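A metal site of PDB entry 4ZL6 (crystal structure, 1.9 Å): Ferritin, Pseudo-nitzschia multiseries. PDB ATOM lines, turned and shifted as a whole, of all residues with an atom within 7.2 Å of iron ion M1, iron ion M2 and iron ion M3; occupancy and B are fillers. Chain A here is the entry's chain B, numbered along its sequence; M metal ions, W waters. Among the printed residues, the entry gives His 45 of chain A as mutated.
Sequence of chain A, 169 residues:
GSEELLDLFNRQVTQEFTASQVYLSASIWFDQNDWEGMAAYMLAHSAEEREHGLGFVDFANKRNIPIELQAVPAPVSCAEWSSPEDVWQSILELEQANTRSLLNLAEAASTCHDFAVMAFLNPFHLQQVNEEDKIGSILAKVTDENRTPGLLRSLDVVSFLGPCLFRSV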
ATOM      1  N   GLN A  12      33.151   0.064  13.291  1.00  0.00           N
ATOM      2  CA  GLN A  12      31.876   0.348  12.689  1.00  0.00           C
ATOM      3  C   GLN A  12      31.021   1.220  13.593  1.00  0.00           C
ATOM      4  O   GLN A  12      30.294   2.084  13.103  1.00  0.00           O
ATOM      5  CB  GLN A  12      31.131  -0.944  12.364  1.00  0.00           C
ATOM      6  CG  GLN A  12      29.890  -0.749  11.535  1.00  0.00           C
ATOM      7  CD  GLN A  12      30.270  -0.200  10.174  1.00  0.00           C
ATOM      8  OE1 GLN A  12      31.338  -0.532   9.593  1.00  0.00           O
ATOM      9  NE2 GLN A  12      29.453   0.674   9.681  1.00  0.00           N
ATOM     10  N   GLN A  15      32.230   4.595  13.062  1.00  0.00           N
ATOM     11  CA  GLN A  15      31.784   5.085  11.776  1.00  0.00           C
ATOM     12  C   GLN A  15      30.345   5.618  11.846  1.00  0.00           C
ATOM     13  O   GLN A  15      30.080   6.662  11.265  1.00  0.00           O
ATOM     14  CB  GLN A  15      31.961   4.082  10.602  1.00  0.00           C
ATOM     15  CG  GLN A  15      33.426   3.953  10.190  1.00  0.00           C
ATOM     16  CD  GLN A  15      34.017   5.333   9.941  1.00  0.00           C
ATOM     17  OE1 GLN A  15      33.561   6.009   9.013  1.00  0.00           O
ATOM     18  NE2 GLN A  15      34.900   5.838  10.898  1.00  0.00           N
ATOM     19  N   GLU A  16      29.438   4.874  12.507  1.00  0.00           N
ATOM     20  CA  GLU A  16      28.043   5.300  12.605  1.00  0.00           C
ATOM     21  C   GLU A  16      27.881   6.592  13.418  1.00  0.00           C
ATOM     22  O   GLU A  16      27.169   7.495  12.972  1.00  0.00           O
ATOM     23  CB  GLU A  16      27.224   4.231  13.266  1.00  0.00           C
ATOM     24  CG  GLU A  16      27.128   2.920  12.549  1.00  0.00           C
ATOM     25  CD  GLU A  16      26.608   3.006  11.120  1.00  0.00           C
ATOM     26  OE1 GLU A  16      25.812   3.908  10.781  1.00  0.00           O
ATOM     27  OE2 GLU A  16      26.990   2.111  10.348  1.00  0.00           O
ATOM     28  N   ALA A  19      29.240   9.411  11.301  1.00  0.00           N
ATOM     29  CA  ALA A  19      28.230   9.801  10.321  1.00  0.00           C
ATOM     30  C   ALA A  19      27.103  10.565  10.997  1.00  0.00           C
ATOM     31  O   ALA A  19      26.614  11.565  10.447  1.00  0.00           O
ATOM     32  CB  ALA A  19      27.695   8.570   9.545  1.00  0.00           C
ATOM     33  N   SER A  20      26.726  10.191  12.236  1.00  0.00           N
ATOM     34  CA  SER A  20      25.701  10.955  12.903  1.00  0.00           C
ATOM     35  C   SER A  20      26.065  12.457  13.052  1.00  0.00           C
ATOM     36  O   SER A  20      25.226  13.384  12.819  1.00  0.00           O
ATOM     37  CB  SER A  20      25.411  10.297  14.270  1.00  0.00           C
ATOM     38  OG  SER A  20      24.439  11.005  14.899  1.00  0.00           O
ATOM     39  N   TYR A  23      26.010  14.287   9.585  1.00  0.00           N
ATOM     40  CA  TYR A  23      24.630  14.631   9.263  1.00  0.00           C
ATOM     41  C   TYR A  23      24.167  15.828  10.086  1.00  0.00           C
ATOM     42  O   TYR A  23      23.506  16.745   9.542  1.00  0.00           O
ATOM     43  CB  TYR A  23      23.668  13.432   9.470  1.00  0.00           C
ATOM     44  CG  TYR A  23      23.543  12.515   8.299  1.00  0.00           C
ATOM     45  CD1 TYR A  23      22.802  12.882   7.184  1.00  0.00           C
ATOM     46  CD2 TYR A  23      24.148  11.276   8.297  1.00  0.00           C
ATOM     47  CE1 TYR A  23      22.638  12.042   6.082  1.00  0.00           C
ATOM     48  CE2 TYR A  23      24.063  10.464   7.166  1.00  0.00           C
ATOM     49  CZ  TYR A  23      23.274  10.827   6.114  1.00  0.00           C
ATOM     50  OH  TYR A  23      23.127   9.991   5.081  1.00  0.00           O
ATOM     51  N   TYR A  41      15.627  16.851   7.072  1.00  0.00           N
ATOM     52  CA  TYR A  41      16.010  15.553   6.590  1.00  0.00           C
ATOM     53  C   TYR A  41      17.386  15.129   7.202  1.00  0.00           C
ATOM     54  O   TYR A  41      17.574  13.998   7.671  1.00  0.00           O
ATOM     55  CB  TYR A  41      16.106  15.546   5.081  1.00  0.00           C
ATOM     56  CG  TYR A  41      16.687  14.313   4.526  1.00  0.00           C
ATOM     57  CD1 TYR A  41      18.058  14.179   4.435  1.00  0.00           C
ATOM     58  CD2 TYR A  41      15.886  13.253   4.146  1.00  0.00           C
ATOM     59  CE1 TYR A  41      18.628  13.031   3.983  1.00  0.00           C
ATOM     60  CE2 TYR A  41      16.456  12.081   3.660  1.00  0.00           C
ATOM     61  CZ  TYR A  41      17.807  11.974   3.585  1.00  0.00           C
ATOM     62  OH  TYR A  41      18.415  10.843   3.169  1.00  0.00           O
ATOM     63  N   HIS A  45      18.210  11.921   9.725  1.00  0.00           N
ATOM     64  CA  HIS A  45      19.144  10.917   9.330  1.00  0.00           C
ATOM     65  C   HIS A  45      20.289  10.868  10.403  1.00  0.00           C
ATOM     66  O   HIS A  45      20.800   9.816  10.693  1.00  0.00           O
ATOM     67  CB  HIS A  45      19.693  11.214   7.947  1.00  0.00           C
ATOM     68  CG  HIS A  45      20.179   9.996   7.244  1.00  0.00           C
ATOM     69  ND1 HIS A  45      19.748   9.653   5.978  1.00  0.00           N
ATOM     70  CD2 HIS A  45      20.970   8.968   7.674  1.00  0.00           C
ATOM     71  CE1 HIS A  45      20.352   8.529   5.612  1.00  0.00           C
ATOM     72  NE2 HIS A  45      21.042   8.066   6.648  1.00  0.00           N
ATOM     73  N   GLU A  48      19.069   8.566  13.009  1.00  0.00           N
ATOM     74  CA  GLU A  48      19.073   7.227  12.484  1.00  0.00           C
ATOM     75  C   GLU A  48      20.480   6.606  12.476  1.00  0.00           C
ATOM     76  O   GLU A  48      20.645   5.403  12.785  1.00  0.00           O
ATOM     77  CB  GLU A  48      18.537   7.234  11.026  1.00  0.00           C
ATOM     78  CG  GLU A  48      18.725   5.858  10.416  1.00  0.00           C
ATOM     79  CD  GLU A  48      17.971   5.668   9.104  1.00  0.00           C
ATOM     80  OE1 GLU A  48      18.211   6.454   8.140  1.00  0.00           O
ATOM     81  OE2 GLU A  48      17.177   4.702   9.046  1.00  0.00           O
ATOM     82  N   GLU A  49      21.498   7.403  12.130  1.00  0.00           N
ATOM     83  CA  GLU A  49      22.850   6.839  12.174  1.00  0.00           C
ATOM     84  C   GLU A  49      23.231   6.466  13.630  1.00  0.00           C
ATOM     85  O   GLU A  49      23.909   5.503  13.899  1.00  0.00           O
ATOM     86  CB  GLU A  49      23.878   7.839  11.735  1.00  0.00           C
ATOM     87  CG  GLU A  49      23.699   8.254  10.337  1.00  0.00           C
ATOM     88  CD  GLU A  49      23.931   7.131   9.337  1.00  0.00           C
ATOM     89  OE1 GLU A  49      24.506   6.085   9.567  1.00  0.00           O
ATOM     90  OE2 GLU A  49      23.637   7.403   8.247  1.00  0.00           O
ATOM     91  N   ARG A  50      22.834   7.324  14.552  1.00  0.00           N
ATOM     92  CA  ARG A  50      23.078   7.032  15.964  1.00  0.00           C
ATOM     93  C   ARG A  50      22.391   5.728  16.336  1.00  0.00           C
ATOM     94  O   ARG A  50      22.977   4.871  17.029  1.00  0.00           O
ATOM     95  CB  ARG A  50      22.591   8.139  16.873  1.00  0.00           C
ATOM     96  CG  ARG A  50      22.999   7.908  18.337  1.00  0.00           C
ATOM     97  CD  ARG A  50      23.017   9.175  19.200  1.00  0.00           C
ATOM     98  NE  ARG A  50      23.152   8.838  20.629  1.00  0.00           N
ATOM     99  CZ  ARG A  50      22.125   8.343  21.344  1.00  0.00           C
ATOM    100  NH1 ARG A  50      20.936   8.151  20.835  1.00  0.00           N
ATOM    101  NH2 ARG A  50      22.328   7.952  22.558  1.00  0.00           N
ATOM    102  N   HIS A  52      21.766   3.124  14.414  1.00  0.00           N
ATOM    103  CA  HIS A  52      22.621   2.097  13.890  1.00  0.00           C
ATOM    104  C   HIS A  52      23.807   1.788  14.771  1.00  0.00           C
ATOM    105  O   HIS A  52      24.098   0.592  15.067  1.00  0.00           O
ATOM    106  CB  HIS A  52      23.180   2.404  12.508  1.00  0.00           C
ATOM    107  CG  HIS A  52      22.132   2.618  11.484  1.00  0.00           C
ATOM    108  ND1 HIS A  52      20.870   2.084  11.608  1.00  0.00           N
ATOM    109  CD2 HIS A  52      22.155   3.328  10.323  1.00  0.00           C
ATOM    110  CE1 HIS A  52      20.145   2.454  10.561  1.00  0.00           C
ATOM    111  NE2 HIS A  52      20.899   3.187   9.770  1.00  0.00           N
ATOM    112  N   GLY A  53      24.518   2.817  15.214  1.00  0.00           N
ATOM    113  CA  GLY A  53      25.574   2.531  16.127  1.00  0.00           C
ATOM    114  C   GLY A  53      25.124   1.824  17.408  1.00  0.00           C
ATOM    115  O   GLY A  53      25.778   0.913  17.886  1.00  0.00           O
ATOM    116  N   PHE A  56      24.693  -1.848  16.767  1.00  0.00           N
ATOM    117  CA  PHE A  56      25.953  -2.549  16.791  1.00  0.00           C
ATOM    118  C   PHE A  56      26.405  -2.765  18.198  1.00  0.00           C
ATOM    119  O   PHE A  56      26.928  -3.854  18.520  1.00  0.00           O
ATOM    120  CB  PHE A  56      26.994  -1.835  15.984  1.00  0.00           C
ATOM    121  CG  PHE A  56      26.894  -2.149  14.478  1.00  0.00           C
ATOM    122  CD1 PHE A  56      25.891  -1.607  13.702  1.00  0.00           C
ATOM    123  CD2 PHE A  56      27.729  -3.067  13.888  1.00  0.00           C
ATOM    124  CE1 PHE A  56      25.720  -1.925  12.363  1.00  0.00           C
ATOM    125  CE2 PHE A  56      27.580  -3.383  12.524  1.00  0.00           C
ATOM    126  CZ  PHE A  56      26.568  -2.828  11.782  1.00  0.00           C
ATOM    127  N   LEU A  94      29.821   9.965   2.291  1.00  0.00           N
ATOM    128  CA  LEU A  94      29.787   9.445   3.652  1.00  0.00           C
ATOM    129  C   LEU A  94      29.088   8.094   3.619  1.00  0.00           C
ATOM    130  O   LEU A  94      29.511   7.118   4.250  1.00  0.00           O
ATOM    131  CB  LEU A  94      29.016  10.472   4.501  1.00  0.00           C
ATOM    132  CG  LEU A  94      28.763  10.113   5.958  1.00  0.00           C
ATOM    133  CD1 LEU A  94      30.045  10.162   6.743  1.00  0.00           C
ATOM    134  CD2 LEU A  94      27.706  10.976   6.572  1.00  0.00           C
ATOM    135  N   GLU A  95      27.945   8.022   2.941  1.00  0.00           N
ATOM    136  CA  GLU A  95      27.259   6.750   2.822  1.00  0.00           C
ATOM    137  C   GLU A  95      28.015   5.709   2.042  1.00  0.00           C
ATOM    138  O   GLU A  95      28.012   4.523   2.404  1.00  0.00           O
ATOM    139  CB  GLU A  95      25.831   6.932   2.310  1.00  0.00           C
ATOM    140  CG  GLU A  95      24.891   7.625   3.298  1.00  0.00           C
ATOM    141  CD  GLU A  95      24.520   6.828   4.526  1.00  0.00           C
ATOM    142  OE1 GLU A  95      24.913   5.649   4.647  1.00  0.00           O
ATOM    143  OE2 GLU A  95      23.794   7.390   5.388  1.00  0.00           O
ATOM    144  N   ASN A  98      30.349   4.411   4.536  1.00  0.00           N
ATOM    145  CA  ASN A  98      29.634   3.572   5.512  1.00  0.00           C
ATOM    146  C   ASN A  98      29.488   2.147   4.818  1.00  0.00           C
ATOM    147  O   ASN A  98      29.724   1.108   5.422  1.00  0.00           O
ATOM    148  CB  ASN A  98      28.192   4.078   5.914  1.00  0.00           C
ATOM    149  CG  ASN A  98      28.086   5.355   6.854  1.00  0.00           C
ATOM    150  OD1 ASN A  98      29.045   5.804   7.489  1.00  0.00           O
ATOM    151  ND2 ASN A  98      26.830   5.921   6.972  1.00  0.00           N
ATOM    152  N   LEU A 102      30.995  -1.518   6.062  1.00  0.00           N
ATOM    153  CA  LEU A 102      30.138  -2.694   6.361  1.00  0.00           C
ATOM    154  C   LEU A 102      30.588  -3.899   5.614  1.00  0.00           C
ATOM    155  O   LEU A 102      30.535  -5.047   6.116  1.00  0.00           O
ATOM    156  CB  LEU A 102      28.678  -2.435   6.005  1.00  0.00           C
ATOM    157  CG  LEU A 102      27.878  -1.684   7.019  1.00  0.00           C
ATOM    158  CD1 LEU A 102      26.530  -1.388   6.351  1.00  0.00           C
ATOM    159  CD2 LEU A 102      27.670  -2.497   8.285  1.00  0.00           C
ATOM    160  N   PHE A 124      21.456  -4.506   7.311  1.00  0.00           N
ATOM    161  CA  PHE A 124      22.230  -3.310   7.090  1.00  0.00           C
ATOM    162  C   PHE A 124      22.789  -3.272   5.647  1.00  0.00           C
ATOM    163  O   PHE A 124      22.897  -2.175   5.063  1.00  0.00           O
ATOM    164  CB  PHE A 124      23.405  -3.253   8.063  1.00  0.00           C
ATOM    165  CG  PHE A 124      22.988  -3.109   9.498  1.00  0.00           C
ATOM    166  CD1 PHE A 124      22.697  -1.844   9.999  1.00  0.00           C
ATOM    167  CD2 PHE A 124      22.847  -4.222  10.342  1.00  0.00           C
ATOM    168  CE1 PHE A 124      22.275  -1.701  11.331  1.00  0.00           C
ATOM    169  CE2 PHE A 124      22.408  -4.093  11.679  1.00  0.00           C
ATOM    170  CZ  PHE A 124      22.113  -2.840  12.151  1.00  0.00           C
ATOM    171  N   GLN A 127      19.740  -2.037   3.723  1.00  0.00           N
ATOM    172  CA  GLN A 127      19.480  -0.644   4.030  1.00  0.00           C
ATOM    173  C   GLN A 127      20.473   0.284   3.307  1.00  0.00           C
ATOM    174  O   GLN A 127      20.024   1.330   2.784  1.00  0.00           O
ATOM    175  CB  GLN A 127      19.561  -0.374   5.549  1.00  0.00           C
ATOM    176  CG  GLN A 127      19.460   1.139   5.882  1.00  0.00           C
ATOM    177  CD  GLN A 127      18.763   1.470   7.227  1.00  0.00           C
ATOM    178  OE1 GLN A 127      18.580   2.657   7.550  1.00  0.00           O
ATOM    179  NE2 GLN A 127      18.387   0.437   8.008  1.00  0.00           N
ATOM    180  N   GLN A 128      21.750  -0.051   3.306  1.00  0.00           N
ATOM    181  CA  GLN A 128      22.754   0.787   2.638  1.00  0.00           C
ATOM    182  C   GLN A 128      22.424   0.918   1.143  1.00  0.00           C
ATOM    183  O   GLN A 128      22.599   1.997   0.566  1.00  0.00           O
ATOM    184  CB  GLN A 128      24.191   0.309   2.817  1.00  0.00           C
ATOM    185  CG  GLN A 128      24.723   0.566   4.200  1.00  0.00           C
ATOM    186  CD  GLN A 128      24.620   2.038   4.549  1.00  0.00           C
ATOM    187  OE1 GLN A 128      23.775   2.456   5.357  1.00  0.00           O
ATOM    188  NE2 GLN A 128      25.372   2.855   3.819  1.00  0.00           N
ATOM    189  N   GLU A 131      19.646   3.498   0.949  1.00  0.00           N
ATOM    190  CA  GLU A 131      20.120   4.855   1.291  1.00  0.00           C
ATOM    191  C   GLU A 131      20.957   5.479   0.225  1.00  0.00           C
ATOM    192  O   GLU A 131      20.733   6.652  -0.087  1.00  0.00           O
ATOM    193  CB  GLU A 131      20.897   4.841   2.615  1.00  0.00           C
ATOM    194  CG  GLU A 131      19.901   4.665   3.720  1.00  0.00           C
ATOM    195  CD  GLU A 131      20.536   4.764   5.085  1.00  0.00           C
ATOM    196  OE1 GLU A 131      21.634   5.303   5.139  1.00  0.00           O
ATOM    197  OE2 GLU A 131      19.917   4.271   6.037  1.00  0.00           O
ATOM    198  N   ILE A 135      19.856   8.889  -1.646  1.00  0.00           N
ATOM    199  CA  ILE A 135      20.723  10.066  -1.546  1.00  0.00           C
ATOM    200  C   ILE A 135      21.162  10.463  -2.946  1.00  0.00           C
ATOM    201  O   ILE A 135      21.091  11.645  -3.322  1.00  0.00           O
ATOM    202  CB  ILE A 135      21.953   9.826  -0.680  1.00  0.00           C
ATOM    203  CG1 ILE A 135      21.535   9.530   0.771  1.00  0.00           C
ATOM    204  CG2 ILE A 135      22.885  11.025  -0.756  1.00  0.00           C
ATOM    205  CD1 ILE A 135      20.901  10.679   1.499  1.00  0.00           C
HETATM  206 FE    FE M   1      22.562   6.284   6.800  1.00  0.00          FE
HETATM  207 FE    FE M   2      20.577   3.548   7.813  1.00  0.00          FE
HETATM  208 FE    FE M   3      24.666   4.152   9.002  1.00  0.00          FE
HETATM  209  O   HOH W   1      21.118   5.665   8.146  1.00  0.00           O
HETATM  210  O   HOH W   2      25.003   1.930   8.474  1.00  0.00           O
HETATM  211  O   HOH W   3      23.878   4.508   6.862  1.00  0.00           O
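The side-chain carboxylate of Glu 49 sits close to the side-chain amide nitrogen of Asn 98. The side-chain carboxylate (OE2) of Glu 16 sits at hydrogen-bond distance from the side-chain amide nitrogen (NE2) of Gln 12 (2.9 Å). OE1 of Glu 95 lies within hydrogen-bond range of ND2 of Asn 98 (3.0 Å). The side-chain amide nitrogen (NE2) of Gln 128 lies within hydrogen-bond range of the side-chain carboxylate (OE1) of Glu 95 (3.0 Å). OE2 of Glu 95 sits close to OH of Tyr 23 (2.7 Å). OE1 of Gln 127 sits close to OE2 of Glu 48, 2.9 Å away. NE2 of His 45 lies close to OH of Tyr 23 (3.2 Å). ND1 of His 45 lies within hydrogen-bond range of OH of Tyr 41 (3.3 Å).
Water W3 lies within hydrogen-bond range of OE1 of Gln 128, OE1 of Glu 95 and ND2 of Asn 98. Water W2 lies within hydrogen-bond range of the side-chain carboxylate of Glu 16 (2.7 Å) and the side-chain amide oxygen of Gln 128 (3.4 Å).
Iron ion M3 is bound by the side-chain carboxylate of Glu 49 (2.0 Å), the side-chain carboxylate of Glu 16 (2.1 Å), water W2 (2.3 Å) and water W3 (2.3 Å).
Four residues have an atom within 4 Å of iron ion M1: His 45, Glu 49, Glu 95 and Glu 131. The nearest printed residue that does not touch iron ion M1 is Tyr 23 (4.1 Å).
Iron ion M2 is bound by NE2 of His 52, OE2 of Glu 131, OE1 of Gln 127 and water W1. Iron ion M2 has four donor atoms within binding distance.
Iron ion M1 is bound by water W1 (2.1 Å), OE2 of Glu 49 (2.1 Å), OE1 of Glu 131 (2.1 Å), OE2 of Glu 95 (2.2 Å), water W3 (2.2 Å) and NE2 of His 45 (2.3 Å). Iron ion M1 has six donor atoms within binding distance.
Residues that only touch iron ion M2: Glu 48. Four residues have an atom within 4 Å of iron ion M2: Glu 48, His 52, Gln 127 and Glu 131.
Asn 98 touches iron ion M3 (ND2 to FE, 3.5 Å). Within 4 Å of iron ion M3: Glu 16, Glu 49, His 52 and Asn 98.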
